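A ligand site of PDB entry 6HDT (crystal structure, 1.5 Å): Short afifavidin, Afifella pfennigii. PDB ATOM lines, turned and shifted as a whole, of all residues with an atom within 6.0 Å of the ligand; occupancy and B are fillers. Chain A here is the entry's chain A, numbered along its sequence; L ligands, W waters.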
ATOM      1  N   ASN A  25       4.569  -3.390  17.520  1.00  0.00           N
ATOM      2  CA  ASN A  25       4.369  -3.118  18.940  1.00  0.00           C
ATOM      3  C   ASN A  25       4.213  -1.622  19.201  1.00  0.00           C
ATOM      4  O   ASN A  25       4.169  -0.822  18.268  1.00  0.00           O
ATOM      5  CB  ASN A  25       5.411  -3.820  19.818  1.00  0.00           C
ATOM      6  CG  ASN A  25       6.738  -3.111  19.826  1.00  0.00           C
ATOM      7  OD1 ASN A  25       6.843  -1.977  19.417  1.00  0.00           O
ATOM      8  ND2 ASN A  25       7.768  -3.802  20.312  1.00  0.00           N
ATOM      9  N   GLN A  26       4.070  -1.260  20.475  1.00  0.00           N
ATOM     10  CA  GLN A  26       3.737   0.112  20.894  1.00  0.00           C
ATOM     11  C   GLN A  26       4.877   1.099  20.608  1.00  0.00           C
ATOM     12  O   GLN A  26       4.668   2.301  20.535  1.00  0.00           O
ATOM     13  CB  GLN A  26       3.366   0.146  22.399  1.00  0.00           C
ATOM     14  CG  GLN A  26       4.521  -0.089  23.383  1.00  0.00           C
ATOM     15  CD  GLN A  26       5.087  -1.510  23.368  1.00  0.00           C
ATOM     16  OE1 GLN A  26       4.384  -2.485  23.090  1.00  0.00           O
ATOM     17  NE2 GLN A  26       6.368  -1.640  23.683  1.00  0.00           N
ATOM     18  N   ASP A  27       6.095   0.587  20.462  1.00  0.00           N
ATOM     19  CA  ASP A  27       7.210   1.413  20.083  1.00  0.00           C
ATOM     20  C   ASP A  27       7.512   1.366  18.591  1.00  0.00           C
ATOM     21  O   ASP A  27       8.515   1.915  18.167  1.00  0.00           O
ATOM     22  CB  ASP A  27       8.461   0.993  20.864  1.00  0.00           C
ATOM     23  CG  ASP A  27       8.334   1.323  22.335  1.00  0.00           C
ATOM     24  OD1 ASP A  27       8.016   2.493  22.657  1.00  0.00           O
ATOM     25  OD2 ASP A  27       8.561   0.424  23.165  1.00  0.00           O
ATOM     26  N   SER A  29       8.287  -1.285  16.751  1.00  0.00           N
ATOM     27  CA  SER A  29       9.045  -2.453  16.289  1.00  0.00           C
ATOM     28  C   SER A  29       8.042  -3.339  15.541  1.00  0.00           C
ATOM     29  O   SER A  29       6.830  -3.329  15.821  1.00  0.00           O
ATOM     30  CB  SER A  29       9.756  -3.190  17.423  1.00  0.00           C
ATOM     31  OG  SER A  29      10.671  -2.305  18.064  1.00  0.00           O
ATOM     32  N   TYR A  45      12.418 -10.020  13.259  1.00  0.00           N
ATOM     33  CA  TYR A  45      12.096  -8.928  14.141  1.00  0.00           C
ATOM     34  C   TYR A  45      12.866  -7.692  13.788  1.00  0.00           C
ATOM     35  O   TYR A  45      14.076  -7.747  13.600  1.00  0.00           O
ATOM     36  CB  TYR A  45      12.407  -9.302  15.594  1.00  0.00           C
ATOM     37  CG  TYR A  45      11.668  -8.484  16.625  1.00  0.00           C
ATOM     38  CD1 TYR A  45      12.161  -7.272  17.067  1.00  0.00           C
ATOM     39  CD2 TYR A  45      10.462  -8.947  17.161  1.00  0.00           C
ATOM     40  CE1 TYR A  45      11.477  -6.508  18.026  1.00  0.00           C
ATOM     41  CE2 TYR A  45       9.787  -8.203  18.114  1.00  0.00           C
ATOM     42  CZ  TYR A  45      10.301  -6.991  18.555  1.00  0.00           C
ATOM     43  OH  TYR A  45       9.644  -6.219  19.483  1.00  0.00           O
ATOM     44  N   VAL A  46      12.155  -6.576  13.712  1.00  0.00           N
ATOM     45  CA  VAL A  46      12.812  -5.298  13.441  1.00  0.00           C
ATOM     46  C   VAL A  46      12.593  -4.376  14.602  1.00  0.00           C
ATOM     47  O   VAL A  46      11.475  -3.926  14.858  1.00  0.00           O
ATOM     48  CB  VAL A  46      12.377  -4.647  12.115  1.00  0.00           C
ATOM     49  CG1 VAL A  46      13.110  -3.309  11.927  1.00  0.00           C
ATOM     50  CG2 VAL A  46      12.676  -5.581  10.955  1.00  0.00           C
ATOM     51  N   ASN A  47      13.691  -4.112  15.309  1.00  0.00           N
ATOM     52  CA  ASN A  47      13.654  -3.244  16.472  1.00  0.00           C
ATOM     53  C   ASN A  47      13.664  -1.776  16.057  1.00  0.00           C
ATOM     54  O   ASN A  47      14.532  -1.343  15.301  1.00  0.00           O
ATOM     55  CB  ASN A  47      14.816  -3.580  17.406  1.00  0.00           C
ATOM     56  CG  ASN A  47      15.003  -2.563  18.507  1.00  0.00           C
ATOM     57  OD1 ASN A  47      14.033  -2.123  19.102  1.00  0.00           O
ATOM     58  ND2 ASN A  47      16.265  -2.195  18.782  1.00  0.00           N
ATOM     59  N   ASN A  48      12.661  -1.035  16.538  1.00  0.00           N
ATOM     60  CA  ASN A  48      12.613   0.377  16.258  1.00  0.00           C
ATOM     61  C   ASN A  48      12.501   1.187  17.598  1.00  0.00           C
ATOM     62  O   ASN A  48      12.357   2.402  17.595  1.00  0.00           O
ATOM     63  CB  ASN A  48      11.538   0.635  15.149  1.00  0.00           C
ATOM     64  CG  ASN A  48      11.774  -0.207  13.842  1.00  0.00           C
ATOM     65  OD1 ASN A  48      12.885  -0.269  13.297  1.00  0.00           O
ATOM     66  ND2 ASN A  48      10.706  -0.843  13.323  1.00  0.00           N
ATOM     67  N   ALA A  49      12.660   0.486  18.736  1.00  0.00           N
ATOM     68  CA  ALA A  49      12.527   1.130  20.043  1.00  0.00           C
ATOM     69  C   ALA A  49      13.719   2.018  20.391  1.00  0.00           C
ATOM     70  O   ALA A  49      14.875   1.609  20.247  1.00  0.00           O
ATOM     71  CB  ALA A  49      12.325   0.093  21.131  1.00  0.00           C
ATOM     72  N   GLY A  51      16.573   4.003  22.602  1.00  0.00           N
ATOM     73  CA  GLY A  51      17.374   3.634  23.787  1.00  0.00           C
ATOM     74  C   GLY A  51      17.921   2.220  23.786  1.00  0.00           C
ATOM     75  O   GLY A  51      18.458   1.748  24.788  1.00  0.00           O
ATOM     76  N   PHE A  52      17.768   1.544  22.649  1.00  0.00           N
ATOM     77  CA  PHE A  52      18.331   0.257  22.369  1.00  0.00           C
ATOM     78  C   PHE A  52      19.139   0.359  21.072  1.00  0.00           C
ATOM     79  O   PHE A  52      18.890   1.246  20.210  1.00  0.00           O
ATOM     80  CB  PHE A  52      17.224  -0.779  22.182  1.00  0.00           C
ATOM     81  CG  PHE A  52      16.403  -1.031  23.418  1.00  0.00           C
ATOM     82  CD1 PHE A  52      16.810  -1.962  24.359  1.00  0.00           C
ATOM     83  CD2 PHE A  52      15.228  -0.338  23.620  1.00  0.00           C
ATOM     84  CE1 PHE A  52      16.041  -2.187  25.495  1.00  0.00           C
ATOM     85  CE2 PHE A  52      14.448  -0.563  24.757  1.00  0.00           C
ATOM     86  CZ  PHE A  52      14.845  -1.491  25.689  1.00  0.00           C
ATOM     87  N   GLY A  53      20.101  -0.546  20.935  1.00  0.00           N
ATOM     88  CA  GLY A  53      20.836  -0.695  19.690  1.00  0.00           C
ATOM     89  C   GLY A  53      20.165  -1.634  18.703  1.00  0.00           C
ATOM     90  O   GLY A  53      18.992  -2.028  18.902  1.00  0.00           O
ATOM     91  N   CYS A  54      20.897  -1.988  17.642  1.00  0.00           N
ATOM     92  CA  CYS A  54      20.424  -2.961  16.619  1.00  0.00           C
ATOM     93  C   CYS A  54      19.051  -2.578  16.057  1.00  0.00           C
ATOM     94  O   CYS A  54      18.129  -3.400  15.954  1.00  0.00           O
ATOM     95  CB  CYS A  54      20.425  -4.376  17.182  1.00  0.00           C
ATOM     96  SG  CYS A  54      22.112  -4.933  17.494  1.00  0.00           S
ATOM     97  N   TRP A  76      20.620 -10.858  19.094  1.00  0.00           N
ATOM     98  CA  TRP A  76      20.881  -9.586  18.398  1.00  0.00           C
ATOM     99  C   TRP A  76      22.217  -9.598  17.660  1.00  0.00           C
ATOM    100  O   TRP A  76      23.129  -8.851  18.004  1.00  0.00           O
ATOM    101  CB  TRP A  76      20.724  -8.402  19.354  1.00  0.00           C
ATOM    102  CG  TRP A  76      19.312  -8.346  19.892  1.00  0.00           C
ATOM    103  CD1 TRP A  76      18.892  -8.751  21.106  1.00  0.00           C
ATOM    104  CD2 TRP A  76      18.146  -7.924  19.178  1.00  0.00           C
ATOM    105  NE1 TRP A  76      17.484  -8.609  21.209  1.00  0.00           N
ATOM    106  CE2 TRP A  76      17.034  -8.062  20.044  1.00  0.00           C
ATOM    107  CE3 TRP A  76      17.949  -7.354  17.914  1.00  0.00           C
ATOM    108  CZ2 TRP A  76      15.745  -7.728  19.659  1.00  0.00           C
ATOM    109  CZ3 TRP A  76      16.661  -7.041  17.534  1.00  0.00           C
ATOM    110  CH2 TRP A  76      15.589  -7.194  18.413  1.00  0.00           C
ATOM    111  N   CYS A  83      24.590  -6.513  19.034  1.00  0.00           N
ATOM    112  CA  CYS A  83      24.407  -5.889  20.340  1.00  0.00           C
ATOM    113  C   CYS A  83      24.764  -6.796  21.541  1.00  0.00           C
ATOM    114  O   CYS A  83      24.581  -6.399  22.692  1.00  0.00           O
ATOM    115  CB  CYS A  83      22.963  -5.368  20.424  1.00  0.00           C
ATOM    116  SG  CYS A  83      22.707  -3.996  19.298  1.00  0.00           S
ATOM    117  N   ASN A  84      25.238  -8.014  21.276  1.00  0.00           N
ATOM    118  CA  ASN A  84      25.724  -8.924  22.330  1.00  0.00           C
ATOM    119  C   ASN A  84      24.670  -9.163  23.413  1.00  0.00           C
ATOM    120  O   ASN A  84      24.862  -8.902  24.590  1.00  0.00           O
ATOM    121  CB  ASN A  84      27.030  -8.403  22.924  1.00  0.00           C
ATOM    122  CG  ASN A  84      27.704  -9.415  23.810  1.00  0.00           C
ATOM    123  OD1 ASN A  84      27.551 -10.614  23.613  1.00  0.00           O
ATOM    124  ND2 ASN A  84      28.460  -8.944  24.799  1.00  0.00           N
ATOM    125  N   SER A  85      23.516  -9.641  22.965  1.00  0.00           N
ATOM    126  CA  SER A  85      22.339  -9.709  23.803  1.00  0.00           C
ATOM    127  C   SER A  85      21.343 -10.628  23.138  1.00  0.00           C
ATOM    128  O   SER A  85      21.421 -10.877  21.943  1.00  0.00           O
ATOM    129  CB  SER A  85      21.713  -8.330  23.936  1.00  0.00           C
ATOM    130  OG  SER A  85      21.434  -7.788  22.661  1.00  0.00           O
ATOM    131  N   THR A  87      16.927 -11.495  23.490  1.00  0.00           N
ATOM    132  CA  THR A  87      15.590 -11.277  24.117  1.00  0.00           C
ATOM    133  C   THR A  87      14.671 -12.468  23.882  1.00  0.00           C
ATOM    134  O   THR A  87      14.694 -13.096  22.828  1.00  0.00           O
ATOM    135  CB  THR A  87      14.916 -10.011  23.518  1.00  0.00           C
ATOM    136  OG1 THR A  87      15.785  -8.879  23.626  1.00  0.00           O
ATOM    137  CG2 THR A  87      13.589  -9.662  24.159  1.00  0.00           C
ATOM    138  N   TRP A  89      10.368 -13.225  24.285  1.00  0.00           N
ATOM    139  CA  TRP A  89       9.064 -12.717  24.604  1.00  0.00           C
ATOM    140  C   TRP A  89       8.177 -13.905  24.897  1.00  0.00           C
ATOM    141  O   TRP A  89       8.340 -14.952  24.278  1.00  0.00           O
ATOM    142  CB  TRP A  89       8.467 -12.002  23.392  1.00  0.00           C
ATOM    143  CG  TRP A  89       9.023 -10.691  23.003  1.00  0.00           C
ATOM    144  CD1 TRP A  89       8.474  -9.468  23.213  1.00  0.00           C
ATOM    145  CD2 TRP A  89      10.225 -10.462  22.258  1.00  0.00           C
ATOM    146  NE1 TRP A  89       9.254  -8.495  22.683  1.00  0.00           N
ATOM    147  CE2 TRP A  89      10.336  -9.080  22.082  1.00  0.00           C
ATOM    148  CE3 TRP A  89      11.204 -11.311  21.719  1.00  0.00           C
ATOM    149  CZ2 TRP A  89      11.386  -8.505  21.370  1.00  0.00           C
ATOM    150  CZ3 TRP A  89      12.266 -10.722  21.031  1.00  0.00           C
ATOM    151  CH2 TRP A  89      12.348  -9.353  20.864  1.00  0.00           C
ATOM    152  N   TRP A 106       8.821  -9.591  28.274  1.00  0.00           N
ATOM    153  CA  TRP A 106      10.093  -9.995  27.685  1.00  0.00           C
ATOM    154  C   TRP A 106      11.182  -9.813  28.661  1.00  0.00           C
ATOM    155  O   TRP A 106      11.075  -8.977  29.561  1.00  0.00           O
ATOM    156  CB  TRP A 106      10.412  -9.215  26.393  1.00  0.00           C
ATOM    157  CG  TRP A 106      10.371  -7.701  26.463  1.00  0.00           C
ATOM    158  CD1 TRP A 106       9.353  -6.878  26.021  1.00  0.00           C
ATOM    159  CD2 TRP A 106      11.403  -6.807  26.951  1.00  0.00           C
ATOM    160  NE1 TRP A 106       9.666  -5.571  26.234  1.00  0.00           N
ATOM    161  CE2 TRP A 106      10.923  -5.492  26.774  1.00  0.00           C
ATOM    162  CE3 TRP A 106      12.702  -6.997  27.488  1.00  0.00           C
ATOM    163  CZ2 TRP A 106      11.653  -4.378  27.149  1.00  0.00           C
ATOM    164  CZ3 TRP A 106      13.432  -5.861  27.858  1.00  0.00           C
ATOM    165  CH2 TRP A 106      12.902  -4.577  27.688  1.00  0.00           C
ATOM    166  N   LEU A 108      15.611  -9.617  28.492  1.00  0.00           N
ATOM    167  CA  LEU A 108      16.721  -9.337  27.602  1.00  0.00           C
ATOM    168  C   LEU A 108      18.009  -9.510  28.384  1.00  0.00           C
ATOM    169  O   LEU A 108      18.276  -8.748  29.315  1.00  0.00           O
ATOM    170  CB  LEU A 108      16.628  -7.899  27.146  1.00  0.00           C
ATOM    171  CG  LEU A 108      17.602  -7.329  26.107  1.00  0.00           C
ATOM    172  CD1 LEU A 108      17.007  -6.023  25.626  1.00  0.00           C
ATOM    173  CD2 LEU A 108      19.017  -7.085  26.648  1.00  0.00           C
ATOM    174  N   TYR A 110      21.985  -9.295  28.703  1.00  0.00           N
ATOM    175  CA  TYR A 110      23.012  -8.442  28.110  1.00  0.00           C
ATOM    176  C   TYR A 110      24.172  -8.371  29.072  1.00  0.00           C
ATOM    177  O   TYR A 110      24.118  -8.874  30.209  1.00  0.00           O
ATOM    178  CB  TYR A 110      22.490  -7.030  27.808  1.00  0.00           C
ATOM    179  CG  TYR A 110      22.099  -6.239  29.041  1.00  0.00           C
ATOM    180  CD1 TYR A 110      20.964  -6.540  29.740  1.00  0.00           C
ATOM    181  CD2 TYR A 110      22.909  -5.200  29.535  1.00  0.00           C
ATOM    182  CE1 TYR A 110      20.617  -5.851  30.890  1.00  0.00           C
ATOM    183  CE2 TYR A 110      22.562  -4.499  30.678  1.00  0.00           C
ATOM    184  CZ  TYR A 110      21.395  -4.834  31.350  1.00  0.00           C
ATOM    185  OH  TYR A 110      21.009  -4.168  32.507  1.00  0.00           O
ATOM    186  N   ASP A 123       5.709  -5.790  25.891  1.00  0.00           N
ATOM    187  CA  ASP A 123       5.326  -5.324  24.562  1.00  0.00           C
ATOM    188  C   ASP A 123       3.932  -5.885  24.236  1.00  0.00           C
ATOM    189  O   ASP A 123       3.635  -7.072  24.501  1.00  0.00           O
ATOM    190  CB  ASP A 123       6.266  -5.823  23.456  1.00  0.00           C
ATOM    191  CG  ASP A 123       7.611  -5.138  23.435  1.00  0.00           C
ATOM    192  OD1 ASP A 123       7.781  -4.069  24.074  1.00  0.00           O
ATOM    193  OD2 ASP A 123       8.526  -5.699  22.751  1.00  0.00           O
ATOM    194  N   PHE A 125       1.638  -6.304  20.843  1.00  0.00           N
ATOM    195  CA  PHE A 125       1.725  -6.337  19.424  1.00  0.00           C
ATOM    196  C   PHE A 125       0.335  -6.294  18.855  1.00  0.00           C
ATOM    197  O   PHE A 125      -0.596  -6.864  19.433  1.00  0.00           O
ATOM    198  CB  PHE A 125       2.445  -7.578  18.966  1.00  0.00           C
ATOM    199  CG  PHE A 125       3.893  -7.643  19.379  1.00  0.00           C
ATOM    200  CD1 PHE A 125       4.245  -8.215  20.567  1.00  0.00           C
ATOM    201  CD2 PHE A 125       4.875  -7.113  18.568  1.00  0.00           C
ATOM    202  CE1 PHE A 125       5.602  -8.294  20.963  1.00  0.00           C
ATOM    203  CE2 PHE A 125       6.211  -7.168  18.951  1.00  0.00           C
ATOM    204  CZ  PHE A 125       6.554  -7.743  20.149  1.00  0.00           C
HETATM  205  C1  LIG L   1      19.978  -4.448  22.354  1.00  0.00           C
HETATM  206  O1  LIG L   1      20.689  -5.108  23.125  1.00  0.00           O
HETATM  207  O2  LIG L   1      19.786  -3.216  22.516  1.00  0.00           O
HETATM  208  C2  LIG L   1      19.322  -5.187  21.201  1.00  0.00           C
HETATM  209  C3  LIG L   1      17.961  -4.616  20.824  1.00  0.00           C
HETATM  210  C4  LIG L   1      16.895  -4.891  21.888  1.00  0.00           C
HETATM  211  C5  LIG L   1      15.540  -4.249  21.593  1.00  0.00           C
HETATM  212  C6  LIG L   1      14.549  -4.609  22.700  1.00  0.00           C
HETATM  213  S1  LIG L   1      13.933  -6.281  22.663  1.00  0.00           S
HETATM  214  C7  LIG L   1      12.635  -5.878  23.795  1.00  0.00           C
HETATM  215  C8  LIG L   1      12.177  -4.475  23.411  1.00  0.00           C
HETATM  216  N1  LIG L   1      11.135  -4.488  22.424  1.00  0.00           N
HETATM  217  C9  LIG L   1      11.455  -3.966  21.240  1.00  0.00           C
HETATM  218  O3  LIG L   1      10.665  -3.866  20.283  1.00  0.00           O
HETATM  219  N2  LIG L   1      12.749  -3.578  21.289  1.00  0.00           N
HETATM  220  C10 LIG L   1      13.290  -3.758  22.629  1.00  0.00           C
HETATM  221  O   HOH W   1      21.449  -4.344  25.450  1.00  0.00           O
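Ala 49 touches the ligand.
Phe 52 touches the ligand (CB to O2, 3.6 Å).
CG of Trp 76 touches C2 of the ligand (3.4 Å).
Cys 83 touches the ligand.
CZ2 of Trp 89 touches S1 of the ligand, 3.6 Å away.
CE2 of Trp 106 touches C7 of the ligand (3.5 Å).
CD1 of Leu 108 touches C4 of the ligand (3.9 Å).
Hydrophobic or aromatic side chains within 4 Å of the ligand: Tyr 45, Ala 49, Phe 52, Trp 76, Trp 89, Trp 106 and Leu 108.
Within 4 Å of the ligand: Asn 25, Ser 29, Tyr 45, Asn 47, Ala 49, Phe 52, Gly 53, Trp 76, Cys 83, Ser 85, Thr 87, Trp 89, Trp 106, Leu 108 and Asp 123.
The side-chain carboxylate (OD2) of Asp 123 is in hydrogen-bond range of a nitrogen (N1) of the ligand, 2.9 Å away.
O3 of the ligand sits at hydrogen-bond distance from ND2 of Asn 25 (2.9 Å).
The side-chain hydroxyl of Tyr 45 sits at hydrogen-bond distance from an oxygen (O3) of the ligand, 2.7 Å away.
An oxygen (O2) of the ligand is in hydrogen-bond range of the backbone NH of Gly 53 (3.1 Å).
A nitrogen (N2) of the ligand is in hydrogen-bond range of the side-chain amide oxygen of Asn 47 (2.9 Å).
The side-chain hydroxyl of Ser 85 is in hydrogen-bond range of an oxygen (O1) of the ligand (2.8 Å).
O3 of the ligand is in hydrogen-bond range of OG of Ser 29 (2.7 Å).
The side-chain hydroxyl (OG1) of Thr 87 sits close to a sulfur (S1) of the ligand, at 3.3 Å.
The side-chain carboxylate (OD2) of Asp 123 is in hydrogen-bond range of the indole nitrogen (NE1) of Trp 89.
N of Trp 76 is in hydrogen-bond range of O of Ser 85, at 3.0 Å.
The side-chain hydroxyl (OG) of Ser 29 lies within hydrogen-bond range of the backbone NH (N) of Ala 49.
The backbone NH (N) of Cys 83 sits at hydrogen-bond distance from the backbone carbonyl oxygen (O) of Trp 76.
OG of Ser 29 lies within hydrogen-bond range of N of Asn 48, 2.8 Å away.
OD1 of Asp 123 lies within hydrogen-bond range of NE1 of Trp 106 (3.2 Å).
OD1 of Asn 25 sits at hydrogen-bond distance from N of Ser 29, at 3.1 Å.
The side-chain amide oxygen of Asn 25 is in hydrogen-bond range of the backbone NH of Asp 27.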
